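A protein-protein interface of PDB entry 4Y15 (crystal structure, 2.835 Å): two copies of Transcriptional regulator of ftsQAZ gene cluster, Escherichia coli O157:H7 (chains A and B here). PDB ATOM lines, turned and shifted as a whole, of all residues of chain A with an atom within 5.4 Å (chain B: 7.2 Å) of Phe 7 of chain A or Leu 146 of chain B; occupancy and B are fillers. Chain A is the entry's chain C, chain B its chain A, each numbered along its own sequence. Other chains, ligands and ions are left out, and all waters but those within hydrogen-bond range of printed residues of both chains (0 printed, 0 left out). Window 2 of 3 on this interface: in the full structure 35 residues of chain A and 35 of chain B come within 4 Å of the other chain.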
ATOM      1  N   ASP A   3       2.441  27.593 -16.473  1.00  0.00           N
ATOM      2  CA  ASP A   3       1.320  27.094 -17.270  1.00  0.00           C
ATOM      3  C   ASP A   3       0.796  25.804 -16.643  1.00  0.00           C
ATOM      4  O   ASP A   3      -0.408  25.546 -16.649  1.00  0.00           O
ATOM      5  CB  ASP A   3       1.726  26.855 -18.735  1.00  0.00           C
ATOM      6  CG  ASP A   3       1.799  28.142 -19.550  1.00  0.00           C
ATOM      7  OD1 ASP A   3       1.393  29.206 -19.035  1.00  0.00           O
ATOM      8  OD2 ASP A   3       2.250  28.088 -20.715  1.00  0.00           O
ATOM      9  N   THR A   4       1.702  25.005 -16.084  1.00  0.00           N
ATOM     10  CA  THR A   4       1.334  23.708 -15.524  1.00  0.00           C
ATOM     11  C   THR A   4       0.766  23.799 -14.114  1.00  0.00           C
ATOM     12  O   THR A   4      -0.171  23.072 -13.780  1.00  0.00           O
ATOM     13  CB  THR A   4       2.532  22.751 -15.487  1.00  0.00           C
ATOM     14  OG1 THR A   4       3.730  23.490 -15.226  1.00  0.00           O
ATOM     15  CG2 THR A   4       2.668  22.018 -16.804  1.00  0.00           C
ATOM     16  N   ASP A   5       1.326  24.673 -13.278  1.00  0.00           N
ATOM     17  CA  ASP A   5       0.890  24.729 -11.887  1.00  0.00           C
ATOM     18  C   ASP A   5      -0.478  25.389 -11.758  1.00  0.00           C
ATOM     19  O   ASP A   5      -1.093  25.351 -10.691  1.00  0.00           O
ATOM     20  CB  ASP A   5       1.893  25.507 -11.031  1.00  0.00           C
ATOM     21  CG  ASP A   5       1.616  25.372  -9.544  1.00  0.00           C
ATOM     22  OD1 ASP A   5       1.869  24.284  -8.987  1.00  0.00           O
ATOM     23  OD2 ASP A   5       1.073  26.330  -8.952  1.00  0.00           O
ATOM     24  N   PHE A   6      -0.963  25.985 -12.842  1.00  0.00           N
ATOM     25  CA  PHE A   6      -2.326  26.491 -12.861  1.00  0.00           C
ATOM     26  C   PHE A   6      -3.271  25.316 -13.076  1.00  0.00           C
ATOM     27  O   PHE A   6      -4.297  25.206 -12.410  1.00  0.00           O
ATOM     28  CB  PHE A   6      -2.498  27.557 -13.945  1.00  0.00           C
ATOM     29  CG  PHE A   6      -3.931  27.934 -14.209  1.00  0.00           C
ATOM     30  CD1 PHE A   6      -4.442  29.126 -13.725  1.00  0.00           C
ATOM     31  CD2 PHE A   6      -4.764  27.103 -14.940  1.00  0.00           C
ATOM     32  CE1 PHE A   6      -5.754  29.479 -13.961  1.00  0.00           C
ATOM     33  CE2 PHE A   6      -6.076  27.448 -15.174  1.00  0.00           C
ATOM     34  CZ  PHE A   6      -6.572  28.638 -14.689  1.00  0.00           C
ATOM     35  N   PHE A   7      -2.927  24.453 -14.034  1.00  0.00           N
ATOM     36  CA  PHE A   7      -3.757  23.292 -14.339  1.00  0.00           C
ATOM     37  C   PHE A   7      -3.939  22.400 -13.123  1.00  0.00           C
ATOM     38  O   PHE A   7      -5.018  21.858 -12.900  1.00  0.00           O
ATOM     39  CB  PHE A   7      -3.151  22.455 -15.475  1.00  0.00           C
ATOM     40  CG  PHE A   7      -3.054  23.169 -16.795  1.00  0.00           C
ATOM     41  CD1 PHE A   7      -2.000  22.914 -17.657  1.00  0.00           C
ATOM     42  CD2 PHE A   7      -4.032  24.065 -17.190  1.00  0.00           C
ATOM     43  CE1 PHE A   7      -1.913  23.554 -18.877  1.00  0.00           C
ATOM     44  CE2 PHE A   7      -3.949  24.709 -18.410  1.00  0.00           C
ATOM     45  CZ  PHE A   7      -2.890  24.452 -19.254  1.00  0.00           C
ATOM     46  N   SER A   8      -2.883  22.248 -12.338  1.00  0.00           N
ATOM     47  CA  SER A   8      -2.975  21.495 -11.096  1.00  0.00           C
ATOM     48  C   SER A   8      -3.714  22.287 -10.049  1.00  0.00           C
ATOM     49  O   SER A   8      -4.412  21.708  -9.215  1.00  0.00           O
ATOM     50  CB  SER A   8      -1.609  21.113 -10.569  1.00  0.00           C
ATOM     51  OG  SER A   8      -0.777  22.248 -10.445  1.00  0.00           O
ATOM     52  N   TRP A   9      -3.529  23.605 -10.063  1.00  0.00           N
ATOM     53  CA  TRP A   9      -4.244  24.423  -9.113  1.00  0.00           C
ATOM     54  C   TRP A   9      -5.714  24.161  -9.370  1.00  0.00           C
ATOM     55  O   TRP A   9      -6.431  23.760  -8.436  1.00  0.00           O
ATOM     56  CB  TRP A   9      -3.909  25.910  -9.248  1.00  0.00           C
ATOM     57  CG  TRP A   9      -4.647  26.772  -8.259  1.00  0.00           C
ATOM     58  CD1 TRP A   9      -4.294  27.019  -6.965  1.00  0.00           C
ATOM     59  CD2 TRP A   9      -5.862  27.498  -8.486  1.00  0.00           C
ATOM     60  NE1 TRP A   9      -5.210  27.855  -6.372  1.00  0.00           N
ATOM     61  CE2 TRP A   9      -6.184  28.162  -7.283  1.00  0.00           C
ATOM     62  CE3 TRP A   9      -6.705  27.654  -9.588  1.00  0.00           C
ATOM     63  CZ2 TRP A   9      -7.309  28.975  -7.158  1.00  0.00           C
ATOM     64  CZ3 TRP A   9      -7.824  28.457  -9.457  1.00  0.00           C
ATOM     65  CH2 TRP A   9      -8.116  29.106  -8.254  1.00  0.00           C
ATOM     66  N   ARG A  10      -6.114  24.223 -10.643  1.00  0.00           N
ATOM     67  CA  ARG A  10      -7.494  23.934 -11.033  1.00  0.00           C
ATOM     68  C   ARG A  10      -7.981  22.604 -10.442  1.00  0.00           C
ATOM     69  O   ARG A  10      -9.061  22.536  -9.849  1.00  0.00           O
ATOM     70  CB  ARG A  10      -7.625  23.889 -12.563  1.00  0.00           C
ATOM     71  CG  ARG A  10      -9.030  23.576 -13.069  1.00  0.00           C
ATOM     72  CD  ARG A  10      -9.084  23.629 -14.585  1.00  0.00           C
ATOM     73  NE  ARG A  10     -10.444  23.497 -15.104  1.00  0.00           N
ATOM     74  CZ  ARG A  10     -11.009  22.338 -15.434  1.00  0.00           C
ATOM     75  NH1 ARG A  10     -10.345  21.197 -15.291  1.00  0.00           N
ATOM     76  NH2 ARG A  10     -12.248  22.316 -15.904  1.00  0.00           N
ATOM     77  N   ARG A  11      -7.195  21.549 -10.623  1.00  0.00           N
ATOM     78  CA  ARG A  11      -7.597  20.218 -10.190  1.00  0.00           C
ATOM     79  C   ARG A  11      -7.747  20.099  -8.668  1.00  0.00           C
ATOM     80  O   ARG A  11      -8.623  19.378  -8.201  1.00  0.00           O
ATOM     81  CB  ARG A  11      -6.599  19.192 -10.711  1.00  0.00           C
ATOM     82  CG  ARG A  11      -6.600  19.121 -12.229  1.00  0.00           C
ATOM     83  CD  ARG A  11      -5.465  18.286 -12.775  1.00  0.00           C
ATOM     84  NE  ARG A  11      -5.957  17.064 -13.402  1.00  0.00           N
ATOM     85  CZ  ARG A  11      -5.235  16.287 -14.202  1.00  0.00           C
ATOM     86  NH1 ARG A  11      -3.977  16.600 -14.486  1.00  0.00           N
ATOM     87  NH2 ARG A  11      -5.774  15.194 -14.724  1.00  0.00           N
ATOM     88  N   PHE B   6       0.450  29.945 -23.010  1.00  0.00           N
ATOM     89  CA  PHE B   6      -0.949  29.640 -23.287  1.00  0.00           C
ATOM     90  C   PHE B   6      -1.789  30.902 -23.197  1.00  0.00           C
ATOM     91  O   PHE B   6      -2.664  31.153 -24.026  1.00  0.00           O
ATOM     92  CB  PHE B   6      -1.467  28.589 -22.297  1.00  0.00           C
ATOM     93  CG  PHE B   6      -2.975  28.499 -22.215  1.00  0.00           C
ATOM     94  CD1 PHE B   6      -3.663  27.464 -22.824  1.00  0.00           C
ATOM     95  CD2 PHE B   6      -3.701  29.445 -21.501  1.00  0.00           C
ATOM     96  CE1 PHE B   6      -5.046  27.385 -22.735  1.00  0.00           C
ATOM     97  CE2 PHE B   6      -5.077  29.374 -21.414  1.00  0.00           C
ATOM     98  CZ  PHE B   6      -5.751  28.341 -22.027  1.00  0.00           C
ATOM     99  N   PHE B   7      -1.517  31.685 -22.162  1.00  0.00           N
ATOM    100  CA  PHE B   7      -2.241  32.916 -21.891  1.00  0.00           C
ATOM    101  C   PHE B   7      -2.162  33.818 -23.121  1.00  0.00           C
ATOM    102  O   PHE B   7      -3.058  34.622 -23.375  1.00  0.00           O
ATOM    103  CB  PHE B   7      -1.679  33.586 -20.638  1.00  0.00           C
ATOM    104  CG  PHE B   7      -1.721  32.699 -19.418  1.00  0.00           C
ATOM    105  CD1 PHE B   7      -0.714  32.748 -18.468  1.00  0.00           C
ATOM    106  CD2 PHE B   7      -2.766  31.807 -19.230  1.00  0.00           C
ATOM    107  CE1 PHE B   7      -0.751  31.925 -17.353  1.00  0.00           C
ATOM    108  CE2 PHE B   7      -2.806  30.981 -18.119  1.00  0.00           C
ATOM    109  CZ  PHE B   7      -1.800  31.041 -17.180  1.00  0.00           C
ATOM    110  N   PRO B 144      -1.604  12.322 -28.448  1.00  0.00           N
ATOM    111  CA  PRO B 144      -0.843  13.119 -27.479  1.00  0.00           C
ATOM    112  C   PRO B 144      -1.382  14.550 -27.275  1.00  0.00           C
ATOM    113  O   PRO B 144      -1.208  15.380 -28.170  1.00  0.00           O
ATOM    114  CB  PRO B 144       0.559  13.169 -28.105  1.00  0.00           C
ATOM    115  N   ILE B 145      -1.962  14.839 -26.109  1.00  0.00           N
ATOM    116  CA  ILE B 145      -2.337  16.205 -25.670  1.00  0.00           C
ATOM    117  C   ILE B 145      -2.545  16.127 -24.166  1.00  0.00           C
ATOM    118  O   ILE B 145      -3.051  15.123 -23.658  1.00  0.00           O
ATOM    119  CB  ILE B 145      -3.658  16.815 -26.288  1.00  0.00           C
ATOM    120  CG1 ILE B 145      -3.586  17.082 -27.795  1.00  0.00           C
ATOM    121  CG2 ILE B 145      -4.013  18.164 -25.604  1.00  0.00           C
ATOM    122  CD1 ILE B 145      -2.517  18.079 -28.228  1.00  0.00           C
ATOM    123  N   LEU B 146      -2.161  17.174 -23.448  1.00  0.00           N
ATOM    124  CA  LEU B 146      -2.573  17.304 -22.058  1.00  0.00           C
ATOM    125  C   LEU B 146      -4.046  17.670 -22.037  1.00  0.00           C
ATOM    126  O   LEU B 146      -4.407  18.810 -22.334  1.00  0.00           O
ATOM    127  CB  LEU B 146      -1.750  18.353 -21.317  1.00  0.00           C
ATOM    128  CG  LEU B 146      -2.268  18.646 -19.905  1.00  0.00           C
ATOM    129  CD1 LEU B 146      -2.240  17.393 -19.042  1.00  0.00           C
ATOM    130  CD2 LEU B 146      -1.471  19.757 -19.262  1.00  0.00           C
ATOM    131  N   SER B 147      -4.886  16.703 -21.685  1.00  0.00           N
ATOM    132  CA  SER B 147      -6.334  16.879 -21.724  1.00  0.00           C
ATOM    133  C   SER B 147      -6.803  18.180 -21.080  1.00  0.00           C
ATOM    134  O   SER B 147      -7.752  18.799 -21.554  1.00  0.00           O
ATOM    135  CB  SER B 147      -7.028  15.701 -21.035  1.00  0.00           C
ATOM    136  OG  SER B 147      -6.812  15.726 -19.635  1.00  0.00           O
ATOM    137  N   ASP B 148      -6.115  18.613 -20.028  1.00  0.00           N
ATOM    138  CA  ASP B 148      -6.453  19.871 -19.371  1.00  0.00           C
ATOM    139  C   ASP B 148      -6.336  21.079 -20.291  1.00  0.00           C
ATOM    140  O   ASP B 148      -7.185  21.969 -20.253  1.00  0.00           O
ATOM    141  CB  ASP B 148      -5.552  20.082 -18.154  1.00  0.00           C
ATOM    142  CG  ASP B 148      -5.893  19.153 -17.006  1.00  0.00           C
ATOM    143  OD1 ASP B 148      -6.712  18.231 -17.205  1.00  0.00           O
ATOM    144  OD2 ASP B 148      -5.338  19.345 -15.905  1.00  0.00           O
ATOM    145  N   GLU B 149      -5.301  21.115 -21.123  1.00  0.00           N
ATOM    146  CA  GLU B 149      -5.136  22.236 -22.037  1.00  0.00           C
ATOM    147  C   GLU B 149      -6.185  22.157 -23.141  1.00  0.00           C
ATOM    148  O   GLU B 149      -6.637  23.180 -23.648  1.00  0.00           O
ATOM    149  CB  GLU B 149      -3.728  22.268 -22.635  1.00  0.00           C
ATOM    150  CG  GLU B 149      -3.381  23.611 -23.272  1.00  0.00           C
ATOM    151  CD  GLU B 149      -2.072  23.591 -24.035  1.00  0.00           C
ATOM    152  OE1 GLU B 149      -1.724  22.533 -24.601  1.00  0.00           O
ATOM    153  OE2 GLU B 149      -1.387  24.637 -24.068  1.00  0.00           O
ATOM    154  N   LEU B 150      -6.583  20.940 -23.501  1.00  0.00           N
ATOM    155  CA  LEU B 150      -7.603  20.757 -24.524  1.00  0.00           C
ATOM    156  C   LEU B 150      -8.938  21.284 -24.019  1.00  0.00           C
ATOM    157  O   LEU B 150      -9.594  22.076 -24.694  1.00  0.00           O
ATOM    158  CB  LEU B 150      -7.743  19.284 -24.912  1.00  0.00           C
ATOM    159  CG  LEU B 150      -8.751  19.011 -26.034  1.00  0.00           C
ATOM    160  CD1 LEU B 150      -8.241  19.572 -27.358  1.00  0.00           C
ATOM    161  CD2 LEU B 150      -9.075  17.529 -26.153  1.00  0.00           C
ATOM    162  N   GLN B 151      -9.333  20.830 -22.830  1.00  0.00           N
ATOM    163  CA  GLN B 151     -10.575  21.272 -22.206  1.00  0.00           C
ATOM    164  C   GLN B 151     -10.649  22.790 -22.139  1.00  0.00           C
ATOM    165  O   GLN B 151     -11.676  23.388 -22.464  1.00  0.00           O
ATOM    166  CB  GLN B 151     -10.714  20.699 -20.793  1.00  0.00           C
ATOM    167  CG  GLN B 151     -10.862  19.193 -20.725  1.00  0.00           C
ATOM    168  CD  GLN B 151     -11.059  18.695 -19.304  1.00  0.00           C
ATOM    169  OE1 GLN B 151     -11.827  19.273 -18.534  1.00  0.00           O
ATOM    170  NE2 GLN B 151     -10.369  17.616 -18.953  1.00  0.00           N
ATOM    171  N   LEU B 152      -9.554  23.407 -21.713  1.00  0.00           N
ATOM    172  CA  LEU B 152      -9.502  24.854 -21.573  1.00  0.00           C
ATOM    173  C   LEU B 152      -9.516  25.553 -22.922  1.00  0.00           C
ATOM    174  O   LEU B 152     -10.161  26.588 -23.084  1.00  0.00           O
ATOM    175  CB  LEU B 152      -8.260  25.270 -20.789  1.00  0.00           C
ATOM    176  CG  LEU B 152      -8.571  26.037 -19.504  1.00  0.00           C
ATOM    177  CD1 LEU B 152      -9.298  25.142 -18.509  1.00  0.00           C
ATOM    178  CD2 LEU B 152      -7.302  26.606 -18.895  1.00  0.00           C
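OD2 of Asp 3 of chain A lies within hydrogen-bond range of N of Phe 6 of chain B.
OD2 of Asp 148 of chain B lies within salt-bridge range of NH1 of Arg 11 of chain A (3.4 Å).
The side-chain carboxylate (OD1) of Asp 148 of chain B is in hydrogen-bond range of the side-chain hydroxyl (OG) of Ser 147 of chain B.
Among the printed residues, pairs that only touch across the chains: Phe 7 of chain A with Leu 146 of chain B, Phe 7 of chain A with Asp 148 of chain B, Asp 3 of chain A with Phe 7 of chain B, Phe 7 of chain A with Leu 152 of chain B and Arg 10 of chain A with Leu 152 of chain B.
Of the printed residues of chain B, Asp 3 of chain A touches Phe 6 (3.5 Å) and Phe 7 (3.8 Å).
Asp 5 of chain A touches none of the printed residues of chain B.
Printed residues of chain B within 4 Å of Arg 11 of chain A: Asp 148 (3.3 Å).
Printed residues of chain A within 4 Å of Phe 6 of chain B: Asp 3 (3.5 Å).
Of the printed residues of chain A, Phe 7 of chain B touches Asp 3 (3.8 Å).
Of chain A, only Phe 7 comes within 4 Å of Leu 146 of chain B.
Printed residues of chain A within 4 Å of Asp 148 of chain B: Phe 7 (3.8 Å) and Arg 11 (3.3 Å).
Leu 150 of chain B touches none of the printed residues of chain A.
The nearest residue of chain B that does not touch Phe 7 of chain A is Glu 149 of chain B (4.1 Å).
The nearest printed residue of chain A that does not touch Leu 152 of chain B is Phe 6 of chain A (4.01 Å).
Hydrophobic or aromatic side chains of chain A that line the printed part of chain B: Phe 7.
Hydrophobic or aromatic side chains of chain B that line the printed part of chain A: Phe 7, Leu 146 and Leu 152.
Positions printed for both chains: 6 and 7.
Of the 7 pairs that touch across the chains among the printed residues, none has its exchanged pair printed and touching as well.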
